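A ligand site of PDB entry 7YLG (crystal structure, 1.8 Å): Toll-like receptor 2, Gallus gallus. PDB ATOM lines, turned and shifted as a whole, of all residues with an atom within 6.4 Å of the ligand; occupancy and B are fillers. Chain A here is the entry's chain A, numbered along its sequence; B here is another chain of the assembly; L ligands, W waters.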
ATOM      1  N   ILE A  19      13.998  -3.765   7.308  1.00  0.00           N
ATOM      2  CA  ILE A  19      15.364  -3.983   7.773  1.00  0.00           C
ATOM      3  C   ILE A  19      16.223  -2.762   7.426  1.00  0.00           C
ATOM      4  O   ILE A  19      16.223  -2.271   6.296  1.00  0.00           O
ATOM      5  CB  ILE A  19      15.946  -5.272   7.179  1.00  0.00           C
ATOM      6  CG1 ILE A  19      15.121  -6.445   7.734  1.00  0.00           C
ATOM      7  CG2 ILE A  19      17.417  -5.416   7.538  1.00  0.00           C
ATOM      8  CD1 ILE A  19      15.744  -7.807   7.523  1.00  0.00           C
ATOM      9  N   SER A  20      16.956  -2.277   8.418  1.00  0.00           N
ATOM     10  CA  SER A  20      17.884  -1.168   8.256  1.00  0.00           C
ATOM     11  C   SER A  20      19.299  -1.622   8.611  1.00  0.00           C
ATOM     12  O   SER A  20      19.502  -2.391   9.567  1.00  0.00           O
ATOM     13  CB  SER A  20      17.441  -0.003   9.141  1.00  0.00           C
ATOM     14  OG  SER A  20      18.492   0.876   9.496  1.00  0.00           O
ATOM     15  N   TYR A  21      20.273  -1.153   7.831  1.00  0.00           N
ATOM     16  CA  TYR A  21      21.646  -1.629   7.954  1.00  0.00           C
ATOM     17  C   TYR A  21      22.531  -0.588   7.271  1.00  0.00           C
ATOM     18  O   TYR A  21      22.081   0.140   6.388  1.00  0.00           O
ATOM     19  CB  TYR A  21      21.842  -3.030   7.340  1.00  0.00           C
ATOM     20  CG  TYR A  21      21.450  -3.066   5.879  1.00  0.00           C
ATOM     21  CD1 TYR A  21      20.139  -3.355   5.499  1.00  0.00           C
ATOM     22  CD2 TYR A  21      22.365  -2.732   4.873  1.00  0.00           C
ATOM     23  CE1 TYR A  21      19.762  -3.351   4.155  1.00  0.00           C
ATOM     24  CE2 TYR A  21      22.001  -2.722   3.527  1.00  0.00           C
ATOM     25  CZ  TYR A  21      20.684  -3.021   3.178  1.00  0.00           C
ATOM     26  OH  TYR A  21      20.296  -3.015   1.868  1.00  0.00           O
ATOM     27  N   SER A  22      23.783  -0.558   7.687  1.00  0.00           N
ATOM     28  CA  SER A  22      24.747   0.381   7.137  1.00  0.00           C
ATOM     29  C   SER A  22      25.296  -0.121   5.809  1.00  0.00           C
ATOM     30  O   SER A  22      25.305  -1.313   5.510  1.00  0.00           O
ATOM     31  CB  SER A  22      25.890   0.596   8.127  1.00  0.00           C
ATOM     32  OG  SER A  22      26.752  -0.525   8.105  1.00  0.00           O
ATOM     33  N   GLU A  23      25.752   0.822   4.984  1.00  0.00           N
ATOM     34  CA  GLU A  23      26.434   0.435   3.746  1.00  0.00           C
ATOM     35  C   GLU A  23      27.596  -0.497   4.036  1.00  0.00           C
ATOM     36  O   GLU A  23      27.808  -1.492   3.325  1.00  0.00           O
ATOM     37  CB  GLU A  23      26.908   1.697   3.008  1.00  0.00           C
ATOM     38  N   HIS A  24      28.348  -0.218   5.117  1.00  0.00           N
ATOM     39  CA  HIS A  24      29.474  -1.058   5.513  1.00  0.00           C
ATOM     40  C   HIS A  24      29.046  -2.506   5.724  1.00  0.00           C
ATOM     41  O   HIS A  24      29.801  -3.428   5.394  1.00  0.00           O
ATOM     42  CB  HIS A  24      30.108  -0.490   6.780  1.00  0.00           C
ATOM     43  CG  HIS A  24      31.284  -1.271   7.277  1.00  0.00           C
ATOM     44  ND1 HIS A  24      31.181  -2.258   8.240  1.00  0.00           N
ATOM     45  CD2 HIS A  24      32.606  -1.197   6.967  1.00  0.00           C
ATOM     46  CE1 HIS A  24      32.381  -2.763   8.483  1.00  0.00           C
ATOM     47  NE2 HIS A  24      33.261  -2.143   7.727  1.00  0.00           N
ATOM     48  N   ALA A  26      26.411  -3.999   4.329  1.00  0.00           N
ATOM     49  CA  ALA A  26      25.443  -4.373   3.305  1.00  0.00           C
ATOM     50  C   ALA A  26      25.698  -5.781   2.790  1.00  0.00           C
ATOM     51  O   ALA A  26      24.744  -6.560   2.646  1.00  0.00           O
ATOM     52  CB  ALA A  26      25.500  -3.377   2.135  1.00  0.00           C
ATOM     53  N   TYR A  46      13.026  -3.331   2.472  1.00  0.00           N
ATOM     54  CA  TYR A  46      14.226  -2.535   2.758  1.00  0.00           C
ATOM     55  C   TYR A  46      14.484  -1.551   1.612  1.00  0.00           C
ATOM     56  O   TYR A  46      14.220  -1.867   0.442  1.00  0.00           O
ATOM     57  CB  TYR A  46      15.468  -3.431   3.014  1.00  0.00           C
ATOM     58  CG  TYR A  46      15.924  -4.338   1.864  1.00  0.00           C
ATOM     59  CD1 TYR A  46      15.303  -5.587   1.621  1.00  0.00           C
ATOM     60  CD2 TYR A  46      17.000  -3.969   1.065  1.00  0.00           C
ATOM     61  CE1 TYR A  46      15.741  -6.399   0.594  1.00  0.00           C
ATOM     62  CE2 TYR A  46      17.425  -4.787   0.039  1.00  0.00           C
ATOM     63  CZ  TYR A  46      16.798  -6.004  -0.187  1.00  0.00           C
ATOM     64  OH  TYR A  46      17.245  -6.799  -1.203  1.00  0.00           O
ATOM     65  N   HIS A  47      14.985  -0.360   1.967  1.00  0.00           N
ATOM     66  CA  HIS A  47      14.935   0.777   1.053  1.00  0.00           C
ATOM     67  C   HIS A  47      15.780   0.555  -0.198  1.00  0.00           C
ATOM     68  O   HIS A  47      15.400   0.993  -1.288  1.00  0.00           O
ATOM     69  CB  HIS A  47      15.384   2.048   1.775  1.00  0.00           C
ATOM     70  CG  HIS A  47      14.365   2.567   2.749  1.00  0.00           C
ATOM     71  ND1 HIS A  47      13.013   2.342   2.607  1.00  0.00           N
ATOM     72  CD2 HIS A  47      14.494   3.333   3.854  1.00  0.00           C
ATOM     73  CE1 HIS A  47      12.351   2.930   3.590  1.00  0.00           C
ATOM     74  NE2 HIS A  47      13.240   3.532   4.367  1.00  0.00           N
ATOM     75  N   GLU A  48      16.925  -0.115  -0.062  1.00  0.00           N
ATOM     76  CA  GLU A  48      17.805  -0.293  -1.210  1.00  0.00           C
ATOM     77  C   GLU A  48      17.078  -0.950  -2.386  1.00  0.00           C
ATOM     78  O   GLU A  48      17.283  -0.576  -3.540  1.00  0.00           O
ATOM     79  CB  GLU A  48      19.046  -1.102  -0.795  1.00  0.00           C
ATOM     80  CG  GLU A  48      20.206  -0.927  -1.748  1.00  0.00           C
ATOM     81  CD  GLU A  48      21.481  -1.634  -1.305  1.00  0.00           C
ATOM     82  OE1 GLU A  48      21.648  -1.956  -0.106  1.00  0.00           O
ATOM     83  OE2 GLU A  48      22.328  -1.869  -2.194  1.00  0.00           O
ATOM     84  N   ARG A  49      16.187  -1.898  -2.104  1.00  0.00           N
ATOM     85  CA  ARG A  49      15.361  -2.540  -3.109  1.00  0.00           C
ATOM     86  C   ARG A  49      13.976  -1.919  -3.259  1.00  0.00           C
ATOM     87  O   ARG A  49      13.437  -1.880  -4.372  1.00  0.00           O
ATOM     88  CB  ARG A  49      15.170  -4.041  -2.774  1.00  0.00           C
ATOM     89  CG  ARG A  49      14.458  -4.816  -3.868  1.00  0.00           C
ATOM     90  CD  ARG A  49      14.096  -6.260  -3.433  1.00  0.00           C
ATOM     91  NE  ARG A  49      13.250  -6.205  -2.249  1.00  0.00           N
ATOM     92  CZ  ARG A  49      13.019  -7.220  -1.426  1.00  0.00           C
ATOM     93  NH1 ARG A  49      13.575  -8.406  -1.666  1.00  0.00           N
ATOM     94  NH2 ARG A  49      12.245  -7.045  -0.365  1.00  0.00           N
ATOM     95  N   PHE A  51      12.538   1.141  -1.973  1.00  0.00           N
ATOM     96  CA  PHE A  51      12.288   2.566  -2.070  1.00  0.00           C
ATOM     97  C   PHE A  51      12.444   2.988  -3.527  1.00  0.00           C
ATOM     98  O   PHE A  51      13.489   2.747  -4.143  1.00  0.00           O
ATOM     99  CB  PHE A  51      13.238   3.361  -1.164  1.00  0.00           C
ATOM    100  CG  PHE A  51      12.918   4.831  -1.061  1.00  0.00           C
ATOM    101  CD1 PHE A  51      13.408   5.736  -1.993  1.00  0.00           C
ATOM    102  CD2 PHE A  51      12.180   5.325  -0.001  1.00  0.00           C
ATOM    103  CE1 PHE A  51      13.147   7.119  -1.886  1.00  0.00           C
ATOM    104  CE2 PHE A  51      11.920   6.696   0.125  1.00  0.00           C
ATOM    105  CZ  PHE A  51      12.392   7.598  -0.824  1.00  0.00           C
ATOM    106  N   SER A  78      29.934   0.919  12.511  1.00  0.00           N
ATOM    107  CA  SER A  78      29.695   1.615  11.251  1.00  0.00           C
ATOM    108  C   SER A  78      28.280   2.179  11.182  1.00  0.00           C
ATOM    109  O   SER A  78      28.073   3.274  10.651  1.00  0.00           O
ATOM    110  CB  SER A  78      29.968   0.683  10.068  1.00  0.00           C
ATOM    111  OG  SER A  78      28.985  -0.338  10.007  1.00  0.00           O
ATOM    112  N   PHE A  79      27.300   1.449  11.727  1.00  0.00           N
ATOM    113  CA  PHE A  79      25.930   1.945  11.783  1.00  0.00           C
ATOM    114  C   PHE A  79      25.787   3.110  12.753  1.00  0.00           C
ATOM    115  O   PHE A  79      25.270   4.181  12.395  1.00  0.00           O
ATOM    116  CB  PHE A  79      24.966   0.812  12.189  1.00  0.00           C
ATOM    117  CG  PHE A  79      23.515   1.207  12.124  1.00  0.00           C
ATOM    118  CD1 PHE A  79      22.943   1.951  13.152  1.00  0.00           C
ATOM    119  CD2 PHE A  79      22.737   0.874  11.020  1.00  0.00           C
ATOM    120  CE1 PHE A  79      21.609   2.334  13.088  1.00  0.00           C
ATOM    121  CE2 PHE A  79      21.399   1.271  10.928  1.00  0.00           C
ATOM    122  CZ  PHE A  79      20.837   2.000  11.972  1.00  0.00           C
ATOM    123  N   SER A  82      27.352   6.501  11.669  1.00  0.00           N
ATOM    124  CA  SER A  82      26.941   7.110  10.415  1.00  0.00           C
ATOM    125  C   SER A  82      25.838   8.126  10.644  1.00  0.00           C
ATOM    126  O   SER A  82      24.880   7.868  11.370  1.00  0.00           O
ATOM    127  CB  SER A  82      26.462   6.027   9.437  1.00  0.00           C
ATOM    128  OG  SER A  82      25.720   6.618   8.394  1.00  0.00           O
ATOM    129  N   CYS A  83      25.984   9.279  10.007  1.00  0.00           N
ATOM    130  CA  CYS A  83      24.987  10.342  10.051  1.00  0.00           C
ATOM    131  C   CYS A  83      23.622   9.846   9.549  1.00  0.00           C
ATOM    132  O   CYS A  83      22.592   9.993  10.219  1.00  0.00           O
ATOM    133  CB  CYS A  83      25.509  11.498   9.191  1.00  0.00           C
ATOM    134  SG  CYS A  83      24.564  12.961   9.192  1.00  0.00           S
ATOM    135  N   TRP A  84      23.610   9.211   8.384  1.00  0.00           N
ATOM    136  CA  TRP A  84      22.360   8.730   7.805  1.00  0.00           C
ATOM    137  C   TRP A  84      21.721   7.650   8.663  1.00  0.00           C
ATOM    138  O   TRP A  84      20.502   7.642   8.865  1.00  0.00           O
ATOM    139  CB  TRP A  84      22.618   8.225   6.389  1.00  0.00           C
ATOM    140  CG  TRP A  84      23.335   9.258   5.631  1.00  0.00           C
ATOM    141  CD1 TRP A  84      24.577   9.154   5.073  1.00  0.00           C
ATOM    142  CD2 TRP A  84      22.897  10.602   5.400  1.00  0.00           C
ATOM    143  NE1 TRP A  84      24.925  10.346   4.478  1.00  0.00           N
ATOM    144  CE2 TRP A  84      23.912  11.245   4.668  1.00  0.00           C
ATOM    145  CE3 TRP A  84      21.743  11.310   5.718  1.00  0.00           C
ATOM    146  CZ2 TRP A  84      23.796  12.555   4.262  1.00  0.00           C
ATOM    147  CZ3 TRP A  84      21.635  12.606   5.319  1.00  0.00           C
ATOM    148  CH2 TRP A  84      22.657  13.224   4.602  1.00  0.00           C
ATOM    149  N   CYS A  85      22.524   6.739   9.206  1.00  0.00           N
ATOM    150  CA  CYS A  85      21.956   5.696  10.073  1.00  0.00           C
ATOM    151  C   CYS A  85      21.369   6.302  11.333  1.00  0.00           C
ATOM    152  O   CYS A  85      20.319   5.860  11.813  1.00  0.00           O
ATOM    153  CB  CYS A  85      23.018   4.679  10.426  1.00  0.00           C
ATOM    154  SG  CYS A  85      23.723   3.834   9.029  1.00  0.00           S
ATOM    155  N   GLN A  86      22.023   7.326  11.886  1.00  0.00           N
ATOM    156  CA  GLN A  86      21.459   8.005  13.058  1.00  0.00           C
ATOM    157  C   GLN A  86      20.116   8.632  12.743  1.00  0.00           C
ATOM    158  O   GLN A  86      19.227   8.650  13.599  1.00  0.00           O
ATOM    159  CB  GLN A  86      22.436   9.072  13.573  1.00  0.00           C
ATOM    160  CG  GLN A  86      23.606   8.428  14.300  1.00  0.00           C
ATOM    161  CD  GLN A  86      24.511   9.483  14.924  1.00  0.00           C
ATOM    162  OE1 GLN A  86      24.087  10.600  15.133  1.00  0.00           O
ATOM    163  NE2 GLN A  86      25.760   9.106  15.216  1.00  0.00           N
ATOM    164  N   GLU A  88      18.006   7.504  10.626  1.00  0.00           N
ATOM    165  CA  GLU A  88      17.078   6.371  10.515  1.00  0.00           C
ATOM    166  C   GLU A  88      16.739   5.828  11.904  1.00  0.00           C
ATOM    167  O   GLU A  88      15.568   5.519  12.184  1.00  0.00           O
ATOM    168  CB  GLU A  88      17.710   5.286   9.618  1.00  0.00           C
ATOM    169  CG  GLU A  88      16.762   4.148   9.210  1.00  0.00           C
ATOM    170  CD  GLU A  88      17.194   3.441   7.920  1.00  0.00           C
ATOM    171  OE1 GLU A  88      18.361   3.023   7.830  1.00  0.00           O
ATOM    172  OE2 GLU A  88      16.369   3.327   6.995  1.00  0.00           O
ATOM    173  N   CYS B  83      15.498   9.304   0.036  1.00  0.00           N
ATOM    174  CA  CYS B  83      15.257   8.616   1.296  1.00  0.00           C
ATOM    175  C   CYS B  83      15.987   9.306   2.445  1.00  0.00           C
ATOM    176  O   CYS B  83      15.399   9.649   3.487  1.00  0.00           O
ATOM    177  CB  CYS B  83      15.706   7.167   1.123  1.00  0.00           C
ATOM    178  SG  CYS B  83      15.391   6.085   2.455  1.00  0.00           S
ATOM    179  N   TRP B  84      17.287   9.550   2.270  1.00  0.00           N
ATOM    180  CA  TRP B  84      18.084  10.168   3.319  1.00  0.00           C
ATOM    181  C   TRP B  84      17.617  11.583   3.625  1.00  0.00           C
ATOM    182  O   TRP B  84      17.537  11.985   4.796  1.00  0.00           O
ATOM    183  CB  TRP B  84      19.555  10.149   2.918  1.00  0.00           C
ATOM    184  CG  TRP B  84      19.937   8.782   2.525  1.00  0.00           C
ATOM    185  CD1 TRP B  84      20.386   8.374   1.308  1.00  0.00           C
ATOM    186  CD2 TRP B  84      19.823   7.606   3.338  1.00  0.00           C
ATOM    187  NE1 TRP B  84      20.589   7.015   1.312  1.00  0.00           N
ATOM    188  CE2 TRP B  84      20.257   6.523   2.550  1.00  0.00           C
ATOM    189  CE3 TRP B  84      19.417   7.371   4.654  1.00  0.00           C
ATOM    190  CZ2 TRP B  84      20.293   5.238   3.030  1.00  0.00           C
ATOM    191  CZ3 TRP B  84      19.455   6.096   5.125  1.00  0.00           C
ATOM    192  CH2 TRP B  84      19.882   5.039   4.322  1.00  0.00           C
HETATM  193  N1  LIG L   1      19.349   1.666   3.027  1.00  0.00           N
HETATM  194  C1  LIG L   1      20.406   2.084   2.063  1.00  0.00           C
HETATM  195  C2  LIG L   1      19.829   2.430   0.715  1.00  0.00           C
HETATM  196  O1  LIG L   1      20.608   2.652  -0.245  1.00  0.00           O
HETATM  197  O2  LIG L   1      18.584   2.505   0.614  1.00  0.00           O
HETATM  198  C3  LIG L   1      21.534   1.052   1.941  1.00  0.00           C
HETATM  199  C4  LIG L   1      22.319   0.931   3.243  1.00  0.00           C
HETATM  200  C5  LIG L   1      22.886   2.276   3.638  1.00  0.00           C
HETATM  201  O3  LIG L   1      23.405   3.004   2.796  1.00  0.00           O
HETATM  202  N2  LIG L   1      22.791   2.601   4.926  1.00  0.00           N
HETATM  203  C6  LIG L   1      23.027   3.971   5.360  1.00  0.00           C
HETATM  204  C7  LIG L   1      24.482   4.256   5.633  1.00  0.00           C
HETATM  205  O4  LIG L   1      25.287   3.364   5.857  1.00  0.00           O
HETATM  206  C8  LIG L   1      22.136   4.331   6.550  1.00  0.00           C
HETATM  207  S1  LIG L   1      22.175   3.157   7.929  1.00  0.00           S
HETATM  208  N3  LIG L   1      24.851   5.531   5.617  1.00  0.00           N
HETATM  209  C9  LIG L   1      25.842   6.005   4.667  1.00  0.00           C
HETATM  210  C10 LIG L   1      27.069   6.539   5.364  1.00  0.00           C
HETATM  211  O5  LIG L   1      26.964   7.581   6.047  1.00  0.00           O
HETATM  212  O6  LIG L   1      28.146   5.922   5.244  1.00  0.00           O
HETATM  213  O   HOH W   1      18.257  -0.545   2.519  1.00  0.00           O
HETATM  214  O   HOH W   2      28.431   9.640   8.375  1.00  0.00           O
HETATM  215  O   HOH W   3      19.287   1.305   5.947  1.00  0.00           O
HETATM  216  O   HOH W   4      28.415   2.492   6.296  1.00  0.00           O
HETATM  217  O   HOH W   5      24.221  -0.617   0.730  1.00  0.00           O
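OG of Ser 82 sits at hydrogen-bond distance from O5 of the ligand. SG of Cys 85 is bonded to S1 of the ligand (2.0 Å). N of Glu 23 sits at hydrogen-bond distance from O4 of the ligand. N2 of the ligand lies within hydrogen-bond range of O of Tyr 21, at 2.9 Å. O2 of the ligand sits at hydrogen-bond distance from N of Glu 48 (3.2 Å).
The side-chain hydroxyl (OG) of Ser 22 is in hydrogen-bond range of the side-chain hydroxyl (OG) of Ser 78 (2.9 Å). The backbone NH (N) of Cys 85 sits at hydrogen-bond distance from the side-chain hydroxyl (OG) of Ser 82 (3.3 Å). The side-chain carboxylate (OE1) of Glu 88 is in hydrogen-bond range of the side-chain hydroxyl (OG) of Ser 20. The side-chain carboxylate (OE1) of Glu 48 sits at hydrogen-bond distance from the side-chain hydroxyl (OH) of Tyr 21 (2.6 Å). The side-chain hydroxyl (OG) of Ser 82 lies within hydrogen-bond range of the backbone NH (N) of Trp 84 of chain A (3.3 Å). OG of Ser 22 lies close to N of His 24, at 3.4 Å.
Merely in contact with the ligand: Ser 22, His 47, Phe 79, Trp 84 of chain A, Glu 88 and Trp 84 of chain B. Hydrophobic or aromatic side chains that line the ligand: Tyr 21, His 47, Phe 79, Trp 84 of chain A and Trp 84 of chain B. Of the 22 residues printed, 11 come within 4 Å of the ligand. The nearest printed residue that does not touch the ligand is Cys 83 of chain A (4.4 Å).
Water W1 lies within hydrogen-bond range of N1 of the ligand, N of Glu 48, OH of Tyr 21 and N of His 47. Water W3 lies within hydrogen-bond range of OE1 of Glu 88 (2.7 Å), N1 of the ligand (2.9 Å) and O of Tyr 21 (3.1 Å). Water W4 lies within hydrogen-bond range of N of His 24 (3.0 Å), O4 of the ligand (3.3 Å) and N of Glu 23 (3.4 Å). Water W2 bridges N of Cys 83 of chain A (3.0 Å) and O5 of the ligand (3.4 Å).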
